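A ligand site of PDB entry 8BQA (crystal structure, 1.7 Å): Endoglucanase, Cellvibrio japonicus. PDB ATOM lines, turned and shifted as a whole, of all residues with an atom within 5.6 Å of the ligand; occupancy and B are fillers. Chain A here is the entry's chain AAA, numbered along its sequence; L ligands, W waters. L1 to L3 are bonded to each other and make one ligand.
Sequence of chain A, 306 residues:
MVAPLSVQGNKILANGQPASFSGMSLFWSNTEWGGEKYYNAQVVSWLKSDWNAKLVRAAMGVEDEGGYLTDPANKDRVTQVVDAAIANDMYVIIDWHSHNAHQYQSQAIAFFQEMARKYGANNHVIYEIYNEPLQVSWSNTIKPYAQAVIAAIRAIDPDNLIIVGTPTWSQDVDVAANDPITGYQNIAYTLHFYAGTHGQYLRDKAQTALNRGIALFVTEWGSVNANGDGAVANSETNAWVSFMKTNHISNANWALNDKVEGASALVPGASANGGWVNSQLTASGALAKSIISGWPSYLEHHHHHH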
ATOM      1  N   PHE A  27       5.816   6.661  -6.542  1.00  0.00           N
ATOM      2  CA  PHE A  27       6.843   5.698  -6.127  1.00  0.00           C
ATOM      3  C   PHE A  27       6.375   4.972  -4.872  1.00  0.00           C
ATOM      4  O   PHE A  27       5.365   5.352  -4.215  1.00  0.00           O
ATOM      5  CB  PHE A  27       8.136   6.487  -5.974  1.00  0.00           C
ATOM      6  CG  PHE A  27       9.405   5.692  -5.867  1.00  0.00           C
ATOM      7  CD1 PHE A  27      10.001   5.156  -6.997  1.00  0.00           C
ATOM      8  CD2 PHE A  27      10.032   5.543  -4.649  1.00  0.00           C
ATOM      9  CE1 PHE A  27      11.191   4.445  -6.868  1.00  0.00           C
ATOM     10  CE2 PHE A  27      11.223   4.851  -4.530  1.00  0.00           C
ATOM     11  CZ  PHE A  27      11.829   4.346  -5.641  1.00  0.00           C
ATOM     12  N   TRP A  28       7.151   3.969  -4.478  1.00  0.00           N
ATOM     13  CA  TRP A  28       6.994   3.364  -3.143  1.00  0.00           C
ATOM     14  C   TRP A  28       6.673   4.446  -2.097  1.00  0.00           C
ATOM     15  O   TRP A  28       7.452   5.415  -1.937  1.00  0.00           O
ATOM     16  CB  TRP A  28       8.293   2.671  -2.749  1.00  0.00           C
ATOM     17  CG  TRP A  28       8.723   1.524  -3.597  1.00  0.00           C
ATOM     18  CD1 TRP A  28       9.421   1.544  -4.768  1.00  0.00           C
ATOM     19  CD2 TRP A  28       8.584   0.154  -3.218  1.00  0.00           C
ATOM     20  NE1 TRP A  28       9.686   0.272  -5.186  1.00  0.00           N
ATOM     21  CE2 TRP A  28       9.168  -0.607  -4.257  1.00  0.00           C
ATOM     22  CE3 TRP A  28       7.987  -0.484  -2.123  1.00  0.00           C
ATOM     23  CZ2 TRP A  28       9.244  -1.999  -4.177  1.00  0.00           C
ATOM     24  CZ3 TRP A  28       8.045  -1.856  -2.065  1.00  0.00           C
ATOM     25  CH2 TRP A  28       8.658  -2.598  -3.084  1.00  0.00           C
ATOM     26  N   TRP A  33      12.221   6.305   1.611  1.00  0.00           N
ATOM     27  CA  TRP A  33      12.501   5.821   0.234  1.00  0.00           C
ATOM     28  C   TRP A  33      12.441   6.969  -0.776  1.00  0.00           C
ATOM     29  O   TRP A  33      12.737   6.705  -1.922  1.00  0.00           O
ATOM     30  CB  TRP A  33      11.547   4.687  -0.168  1.00  0.00           C
ATOM     31  CG  TRP A  33      11.910   3.369   0.453  1.00  0.00           C
ATOM     32  CD1 TRP A  33      12.280   3.144   1.754  1.00  0.00           C
ATOM     33  CD2 TRP A  33      11.905   2.087  -0.198  1.00  0.00           C
ATOM     34  NE1 TRP A  33      12.502   1.812   1.957  1.00  0.00           N
ATOM     35  CE2 TRP A  33      12.304   1.135   0.778  1.00  0.00           C
ATOM     36  CE3 TRP A  33      11.631   1.648  -1.493  1.00  0.00           C
ATOM     37  CZ2 TRP A  33      12.399  -0.225   0.486  1.00  0.00           C
ATOM     38  CZ3 TRP A  33      11.747   0.308  -1.785  1.00  0.00           C
ATOM     39  CH2 TRP A  33      12.127  -0.614  -0.811  1.00  0.00           C
ATOM     40  N   ARG A  57      -1.943   6.359  -8.743  1.00  0.00           N
ATOM     41  CA  ARG A  57      -1.735   5.092  -8.002  1.00  0.00           C
ATOM     42  C   ARG A  57      -0.892   5.387  -6.754  1.00  0.00           C
ATOM     43  O   ARG A  57       0.207   5.990  -6.871  1.00  0.00           O
ATOM     44  CB  ARG A  57      -1.078   4.033  -8.913  1.00  0.00           C
ATOM     45  CG  ARG A  57      -0.667   2.736  -8.241  1.00  0.00           C
ATOM     46  CD  ARG A  57      -0.245   1.807  -9.360  1.00  0.00           C
ATOM     47  NE  ARG A  57       0.183   0.451  -9.085  1.00  0.00           N
ATOM     48  CZ  ARG A  57       1.439   0.002  -9.086  1.00  0.00           C
ATOM     49  NH1 ARG A  57       2.484   0.830  -9.146  1.00  0.00           N
ATOM     50  NH2 ARG A  57       1.644  -1.281  -8.915  1.00  0.00           N
ATOM     51  N   ASP A  64       8.537  -4.832   2.519  1.00  0.00           N
ATOM     52  CA  ASP A  64       9.845  -4.151   2.297  1.00  0.00           C
ATOM     53  C   ASP A  64      10.099  -3.118   3.412  1.00  0.00           C
ATOM     54  O   ASP A  64       9.157  -2.448   3.918  1.00  0.00           O
ATOM     55  CB  ASP A  64       9.943  -3.608   0.882  1.00  0.00           C
ATOM     56  CG  ASP A  64       9.913  -4.706  -0.149  1.00  0.00           C
ATOM     57  OD1 ASP A  64       8.808  -5.063  -0.575  1.00  0.00           O
ATOM     58  OD2 ASP A  64      10.999  -5.252  -0.444  1.00  0.00           O
ATOM     59  N   HIS A  97       1.659  -2.863  -2.515  1.00  0.00           N
ATOM     60  CA  HIS A  97       2.842  -2.867  -3.372  1.00  0.00           C
ATOM     61  C   HIS A  97       3.831  -3.914  -2.855  1.00  0.00           C
ATOM     62  O   HIS A  97       4.903  -3.491  -2.344  1.00  0.00           O
ATOM     63  CB  HIS A  97       3.497  -1.494  -3.457  1.00  0.00           C
ATOM     64  CG  HIS A  97       4.381  -1.372  -4.654  1.00  0.00           C
ATOM     65  ND1 HIS A  97       3.859  -1.150  -5.922  1.00  0.00           N
ATOM     66  CD2 HIS A  97       5.727  -1.440  -4.789  1.00  0.00           C
ATOM     67  CE1 HIS A  97       4.855  -1.097  -6.790  1.00  0.00           C
ATOM     68  NE2 HIS A  97       6.017  -1.282  -6.115  1.00  0.00           N
ATOM     69  N   HIS A  99       5.807  -7.922  -3.636  1.00  0.00           N
ATOM     70  CA  HIS A  99       6.181  -9.030  -4.538  1.00  0.00           C
ATOM     71  C   HIS A  99       5.812 -10.401  -3.949  1.00  0.00           C
ATOM     72  O   HIS A  99       6.040 -11.404  -4.652  1.00  0.00           O
ATOM     73  CB  HIS A  99       7.680  -8.981  -4.841  1.00  0.00           C
ATOM     74  CG  HIS A  99       8.073  -7.833  -5.699  1.00  0.00           C
ATOM     75  ND1 HIS A  99       7.571  -7.652  -6.974  1.00  0.00           N
ATOM     76  CD2 HIS A  99       8.901  -6.792  -5.449  1.00  0.00           C
ATOM     77  CE1 HIS A  99       8.116  -6.565  -7.501  1.00  0.00           C
ATOM     78  NE2 HIS A  99       8.924  -6.013  -6.588  1.00  0.00           N
ATOM     79  N   ASN A 131       0.638  -6.119  -6.247  1.00  0.00           N
ATOM     80  CA  ASN A 131       1.455  -5.416  -7.274  1.00  0.00           C
ATOM     81  C   ASN A 131       2.050  -6.388  -8.303  1.00  0.00           C
ATOM     82  O   ASN A 131       1.640  -6.327  -9.518  1.00  0.00           O
ATOM     83  CB  ASN A 131       2.542  -4.625  -6.570  1.00  0.00           C
ATOM     84  CG  ASN A 131       3.618  -4.108  -7.506  1.00  0.00           C
ATOM     85  OD1 ASN A 131       3.307  -3.531  -8.520  1.00  0.00           O
ATOM     86  ND2 ASN A 131       4.876  -4.238  -7.111  1.00  0.00           N
ATOM     87  N   GLU A 132       3.076  -7.131  -7.909  1.00  0.00           N
ATOM     88  CA  GLU A 132       3.927  -7.878  -8.867  1.00  0.00           C
ATOM     89  C   GLU A 132       4.351  -9.220  -8.282  1.00  0.00           C
ATOM     90  O   GLU A 132       5.441  -9.347  -7.724  1.00  0.00           O
ATOM     91  CB  GLU A 132       5.139  -7.031  -9.261  1.00  0.00           C
ATOM     92  CG  GLU A 132       4.897  -6.330 -10.568  1.00  0.00           C
ATOM     93  CD  GLU A 132       6.112  -5.704 -11.183  1.00  0.00           C
ATOM     94  OE1 GLU A 132       7.241  -5.987 -10.716  1.00  0.00           O
ATOM     95  OE2 GLU A 132       5.935  -4.991 -12.177  1.00  0.00           O
ATOM     96  N   HIS A 192       2.046  -5.403 -16.588  1.00  0.00           N
ATOM     97  CA  HIS A 192       3.179  -4.474 -16.339  1.00  0.00           C
ATOM     98  C   HIS A 192       4.198  -4.674 -17.454  1.00  0.00           C
ATOM     99  O   HIS A 192       4.666  -5.812 -17.629  1.00  0.00           O
ATOM    100  CB  HIS A 192       3.785  -4.715 -14.956  1.00  0.00           C
ATOM    101  CG  HIS A 192       2.946  -4.239 -13.815  1.00  0.00           C
ATOM    102  ND1 HIS A 192       3.381  -4.307 -12.509  1.00  0.00           N
ATOM    103  CD2 HIS A 192       1.743  -3.620 -13.760  1.00  0.00           C
ATOM    104  CE1 HIS A 192       2.468  -3.804 -11.693  1.00  0.00           C
ATOM    105  NE2 HIS A 192       1.448  -3.377 -12.433  1.00  0.00           N
ATOM    106  N   TYR A 194       7.802  -2.627 -19.388  1.00  0.00           N
ATOM    107  CA  TYR A 194       8.907  -1.645 -19.333  1.00  0.00           C
ATOM    108  C   TYR A 194       9.524  -1.673 -20.726  1.00  0.00           C
ATOM    109  O   TYR A 194      10.126  -2.716 -21.120  1.00  0.00           O
ATOM    110  CB  TYR A 194       9.839  -1.978 -18.151  1.00  0.00           C
ATOM    111  CG  TYR A 194       9.019  -2.210 -16.896  1.00  0.00           C
ATOM    112  CD1 TYR A 194       8.537  -3.479 -16.587  1.00  0.00           C
ATOM    113  CD2 TYR A 194       8.552  -1.137 -16.167  1.00  0.00           C
ATOM    114  CE1 TYR A 194       7.696  -3.689 -15.514  1.00  0.00           C
ATOM    115  CE2 TYR A 194       7.691  -1.325 -15.085  1.00  0.00           C
ATOM    116  CZ  TYR A 194       7.250  -2.596 -14.775  1.00  0.00           C
ATOM    117  OH  TYR A 194       6.419  -2.785 -13.702  1.00  0.00           O
ATOM    118  N   GLU A 220       1.163  -0.291 -13.755  1.00  0.00           N
ATOM    119  CA  GLU A 220       2.567   0.140 -13.670  1.00  0.00           C
ATOM    120  C   GLU A 220       3.194  -0.127 -15.031  1.00  0.00           C
ATOM    121  O   GLU A 220       3.124  -1.287 -15.490  1.00  0.00           O
ATOM    122  CB  GLU A 220       3.286  -0.648 -12.547  1.00  0.00           C
ATOM    123  CG  GLU A 220       4.743  -0.255 -12.357  1.00  0.00           C
ATOM    124  CD  GLU A 220       5.537  -1.227 -11.482  1.00  0.00           C
ATOM    125  OE1 GLU A 220       4.904  -2.127 -10.868  1.00  0.00           O
ATOM    126  OE2 GLU A 220       6.780  -1.070 -11.372  1.00  0.00           O
ATOM    127  N   ASN A 225      14.118   0.523 -18.782  1.00  0.00           N
ATOM    128  CA  ASN A 225      14.273  -0.933 -18.516  1.00  0.00           C
ATOM    129  C   ASN A 225      13.350  -1.356 -17.356  1.00  0.00           C
ATOM    130  O   ASN A 225      12.874  -0.471 -16.578  1.00  0.00           O
ATOM    131  CB  ASN A 225      15.741  -1.321 -18.298  1.00  0.00           C
ATOM    132  CG  ASN A 225      16.615  -0.866 -19.452  1.00  0.00           C
ATOM    133  OD1 ASN A 225      17.774  -0.463 -19.297  1.00  0.00           O
ATOM    134  ND2 ASN A 225      16.049  -0.908 -20.629  1.00  0.00           N
ATOM    135  N   ALA A 226      13.106  -2.663 -17.225  1.00  0.00           N
ATOM    136  CA  ALA A 226      12.271  -3.263 -16.153  1.00  0.00           C
ATOM    137  C   ALA A 226      12.809  -2.870 -14.764  1.00  0.00           C
ATOM    138  O   ALA A 226      11.997  -2.755 -13.825  1.00  0.00           O
ATOM    139  CB  ALA A 226      12.173  -4.768 -16.297  1.00  0.00           C
ATOM    140  N   ASN A 227      14.115  -2.614 -14.635  1.00  0.00           N
ATOM    141  CA  ASN A 227      14.711  -2.346 -13.307  1.00  0.00           C
ATOM    142  C   ASN A 227      14.494  -0.886 -12.895  1.00  0.00           C
ATOM    143  O   ASN A 227      14.934  -0.552 -11.788  1.00  0.00           O
ATOM    144  CB  ASN A 227      16.174  -2.789 -13.228  1.00  0.00           C
ATOM    145  CG  ASN A 227      17.115  -1.899 -13.998  1.00  0.00           C
ATOM    146  OD1 ASN A 227      16.693  -1.098 -14.817  1.00  0.00           O
ATOM    147  ND2 ASN A 227      18.400  -2.119 -13.797  1.00  0.00           N
ATOM    148  N   GLY A 228      13.822  -0.056 -13.707  1.00  0.00           N
ATOM    149  CA  GLY A 228      13.486   1.335 -13.378  1.00  0.00           C
ATOM    150  C   GLY A 228      14.622   2.295 -13.772  1.00  0.00           C
ATOM    151  O   GLY A 228      14.577   3.486 -13.399  1.00  0.00           O
ATOM    152  N   ASP A 229      15.582   1.803 -14.525  1.00  0.00           N
ATOM    153  CA  ASP A 229      16.708   2.649 -15.004  1.00  0.00           C
ATOM    154  C   ASP A 229      16.933   2.432 -16.497  1.00  0.00           C
ATOM    155  O   ASP A 229      16.221   1.631 -17.093  1.00  0.00           O
ATOM    156  CB  ASP A 229      17.970   2.358 -14.180  1.00  0.00           C
ATOM    157  CG  ASP A 229      18.922   3.546 -14.122  1.00  0.00           C
ATOM    158  OD1 ASP A 229      18.523   4.684 -14.535  1.00  0.00           O
ATOM    159  OD2 ASP A 229      20.065   3.311 -13.697  1.00  0.00           O
ATOM    160  N   TRP A 254       5.256   4.582 -14.156  1.00  0.00           N
ATOM    161  CA  TRP A 254       6.220   4.465 -13.043  1.00  0.00           C
ATOM    162  C   TRP A 254       7.440   5.314 -13.397  1.00  0.00           C
ATOM    163  O   TRP A 254       8.098   4.982 -14.393  1.00  0.00           O
ATOM    164  CB  TRP A 254       6.607   3.008 -12.816  1.00  0.00           C
ATOM    165  CG  TRP A 254       7.473   2.799 -11.613  1.00  0.00           C
ATOM    166  CD1 TRP A 254       8.835   2.860 -11.552  1.00  0.00           C
ATOM    167  CD2 TRP A 254       7.029   2.537 -10.278  1.00  0.00           C
ATOM    168  NE1 TRP A 254       9.266   2.631 -10.279  1.00  0.00           N
ATOM    169  CE2 TRP A 254       8.178   2.439  -9.468  1.00  0.00           C
ATOM    170  CE3 TRP A 254       5.772   2.392  -9.679  1.00  0.00           C
ATOM    171  CZ2 TRP A 254       8.112   2.153  -8.105  1.00  0.00           C
ATOM    172  CZ3 TRP A 254       5.697   2.116  -8.326  1.00  0.00           C
ATOM    173  CH2 TRP A 254       6.857   1.996  -7.555  1.00  0.00           C
ATOM    174  N   LYS A 259      14.257  10.490  -7.713  1.00  0.00           N
ATOM    175  CA  LYS A 259      15.463   9.636  -7.606  1.00  0.00           C
ATOM    176  C   LYS A 259      16.249   9.666  -8.924  1.00  0.00           C
ATOM    177  O   LYS A 259      15.632   9.793  -9.951  1.00  0.00           O
ATOM    178  CB  LYS A 259      14.996   8.205  -7.310  1.00  0.00           C
ATOM    179  CG  LYS A 259      16.085   7.156  -7.430  1.00  0.00           C
ATOM    180  CD  LYS A 259      15.662   5.802  -6.944  1.00  0.00           C
ATOM    181  CE  LYS A 259      16.835   4.850  -7.065  1.00  0.00           C
ATOM    182  NZ  LYS A 259      16.564   3.612  -6.317  1.00  0.00           N
ATOM    183  N   GLU A 261      17.260   7.866 -11.508  1.00  0.00           N
ATOM    184  CA  GLU A 261      17.074   6.634 -12.320  1.00  0.00           C
ATOM    185  C   GLU A 261      16.161   6.997 -13.482  1.00  0.00           C
ATOM    186  O   GLU A 261      15.343   7.889 -13.292  1.00  0.00           O
ATOM    187  CB  GLU A 261      16.490   5.504 -11.452  1.00  0.00           C
ATOM    188  CG  GLU A 261      15.008   5.645 -11.156  1.00  0.00           C
ATOM    189  CD  GLU A 261      14.463   4.566 -10.229  1.00  0.00           C
ATOM    190  OE1 GLU A 261      15.262   3.726  -9.761  1.00  0.00           O
ATOM    191  OE2 GLU A 261      13.259   4.553  -9.994  1.00  0.00           O
ATOM    192  N   ALA A 263      13.452   5.856 -14.666  1.00  0.00           N
ATOM    193  CA  ALA A 263      11.972   5.787 -14.562  1.00  0.00           C
ATOM    194  C   ALA A 263      11.432   7.032 -13.854  1.00  0.00           C
ATOM    195  O   ALA A 263      10.180   7.280 -13.884  1.00  0.00           O
ATOM    196  CB  ALA A 263      11.542   4.513 -13.870  1.00  0.00           C
HETATM  197  O1  LIG L   1       9.749  -3.136 -11.556  1.00  0.00           O
HETATM  198  C1  LIG L   1       8.884  -1.985 -11.651  1.00  0.00           C
HETATM  199  C2  LIG L   1       9.617  -0.802 -11.012  1.00  0.00           C
HETATM  200  C3  LIG L   1      10.898  -0.485 -11.769  1.00  0.00           C
HETATM  201  O2  LIG L   1      10.664  -0.229 -13.155  1.00  0.00           O
HETATM  202  C4  LIG L   1       9.768  -0.990  -9.502  1.00  0.00           C
HETATM  203  O3  LIG L   1      10.360   0.159  -8.858  1.00  0.00           O
HETATM  204  C5  LIG L   1       8.424  -1.238  -8.832  1.00  0.00           C
HETATM  205  O4  LIG L   1       8.628  -1.482  -7.428  1.00  0.00           O
HETATM  206  C6  LIG L   1       7.721  -2.422  -9.470  1.00  0.00           C
HETATM  207  O5  LIG L   1       6.459  -2.634  -8.817  1.00  0.00           O
HETATM  208  C7  LIG L   1       7.531  -2.203 -10.972  1.00  0.00           C
HETATM  209  C1  LG2 L   2      13.740   1.316  -7.863  1.00  0.00           C
HETATM  210  C2  LG2 L   2      12.306   1.428  -8.376  1.00  0.00           C
HETATM  211  C3  LG2 L   2      12.885  -1.471  -5.336  1.00  0.00           C
HETATM  212  C4  LG2 L   2      16.915   0.921  -4.409  1.00  0.00           C
HETATM  213  O1  LG2 L   2      12.231   2.095  -9.634  1.00  0.00           O
HETATM  214  O2  LG2 L   2      17.692   0.168  -5.310  1.00  0.00           O
HETATM  215  O3  LG2 L   2      14.722   1.776  -4.211  1.00  0.00           O
HETATM  216  O4  LG2 L   2      12.772  -2.855  -5.476  1.00  0.00           O
HETATM  217  O5  LG2 L   2      11.716  -0.580  -7.216  1.00  0.00           O
HETATM  218  C5  LG2 L   2      13.055  -0.797  -6.683  1.00  0.00           C
HETATM  219  C6  LG2 L   2      13.759   0.564  -6.544  1.00  0.00           C
HETATM  220  C7  LG2 L   2      15.489   1.055  -4.863  1.00  0.00           C
HETATM  221  C8  LG2 L   2      11.661   0.076  -8.473  1.00  0.00           C
HETATM  222  N1  LG2 L   2      15.098   0.408  -5.973  1.00  0.00           N
HETATM  223  O6  LG2 L   2      14.309   2.605  -7.677  1.00  0.00           O
HETATM  224  C1  LG3 L   3      13.812  -3.675  -5.218  1.00  0.00           C
HETATM  225  C2  LG3 L   3      13.613  -5.112  -5.710  1.00  0.00           C
HETATM  226  C3  LG3 L   3      12.384  -5.734  -4.996  1.00  0.00           C
HETATM  227  C4  LG3 L   3      12.418  -5.546  -3.500  1.00  0.00           C
HETATM  228  C5  LG3 L   3      12.722  -4.117  -3.103  1.00  0.00           C
HETATM  229  O1  LG3 L   3      13.336  -5.205  -7.102  1.00  0.00           O
HETATM  230  O2  LG3 L   3      12.397  -7.109  -5.271  1.00  0.00           O
HETATM  231  O3  LG3 L   3      11.182  -5.963  -2.907  1.00  0.00           O
HETATM  232  O4  LG3 L   3      13.855  -3.632  -3.795  1.00  0.00           O
HETATM  233  O   HOH W   1      11.609  -8.310  -7.897  1.00  0.00           O
HETATM  234  O   HOH W   2       9.324  -5.555 -12.664  1.00  0.00           O
HETATM  235  O   HOH W   3      10.467  -8.571  -2.706  1.00  0.00           O
HETATM  236  O   HOH W   4      10.369  -3.681  -7.162  1.00  0.00           O
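OE2 of Glu 220 is covalently linked to C7 of LIG L1, 1.4 Å away.
The side-chain carboxylate of Glu 261 lies within hydrogen-bond range of an oxygen (O6) of LG2 L2, 2.6 Å away.
The side-chain carboxylate (OD2) of Asp 64 is in hydrogen-bond range of an oxygen (O3) of LG3 L3 (2.6 Å).
An oxygen (O6) of LG2 L2 is in hydrogen-bond range of the side-chain amino group (NZ) of Lys 259, 2.8 Å away.
The side-chain amide nitrogen (ND2) of Asn 131 lies within hydrogen-bond range of an oxygen (O5) of LIG L1, 2.8 Å away.
O4 of LIG L1 is in hydrogen-bond range of NE2 of His 97, 2.9 Å away.
An oxygen (O2) of LIG L1 is in hydrogen-bond range of the backbone carbonyl oxygen (O) of Ala 226 (2.9 Å).
The indole nitrogen (NE1) of Trp 28 sits at hydrogen-bond distance from an oxygen (O5) of LG2 L2 (3.0 Å).
The indole nitrogen (NE1) of Trp 254 lies within hydrogen-bond range of an oxygen (O3) of LIG L1 (3.1 Å).
An oxygen (O2) of LIG L1 lies within hydrogen-bond range of the backbone NH (N) of Gly 228, at 3.2 Å.
Water W2 bridges O1 of LIG L1 and OE1 of Glu 132.
Water W4 lies within hydrogen-bond range of NE2 of His 99 (2.8 Å) and O4 of LIG L1 (2.8 Å).
OD1 of Asn 131 lies close to OE1 of Glu 220 (3.2 Å).
The side-chain carboxylate (OE2) of Glu 220 lies close to the side-chain hydroxyl (OH) of Tyr 194, at 2.9 Å.
The side-chain carboxylate of Glu 220 lies close to a ring nitrogen (ND1) of His 192, 3.1 Å away.
OE1 of Glu 220 is in salt-bridge range of NH2 of Arg 57, at 3.9 Å.
OE1 of Glu 261 lies within salt-bridge range of NZ of Lys 259, at 3.7 Å.
NE2 of His 97 sits close to ND2 of Asn 131 (3.3 Å).
The side-chain amide oxygen (OD1) of Asn 131 is in hydrogen-bond range of the guanidinium group (NH2) of Arg 57 (2.8 Å).
The backbone carbonyl oxygen (O) of Gly 228 is in hydrogen-bond range of the backbone NH (N) of Ala 263 (2.9 Å).
CE1 of Phe 27 touches C2 of LG2 L2, at 3.6 Å.
CD2 of His 99 touches O3 of LG3 L3, at 3.5 Å.
OE2 of Glu 132 touches C7 of LIG L1 (3.4 Å).
OH of Tyr 194 touches C7 of LIG L1 (3.0 Å).
Asn 227 touches the ligand.
Hydrophobic or aromatic side chains that line the ligand: Phe 27, Trp 28, His 97, His 99, Tyr 194 and Trp 254.
15 residues have an atom within 4 Å of the ligand: Phe 27, Trp 28, Asp 64, His 97, His 99, Asn 131, Glu 132, Tyr 194, Glu 220, Ala 226, Asn 227, Gly 228, Trp 254, Lys 259 and Glu 261.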
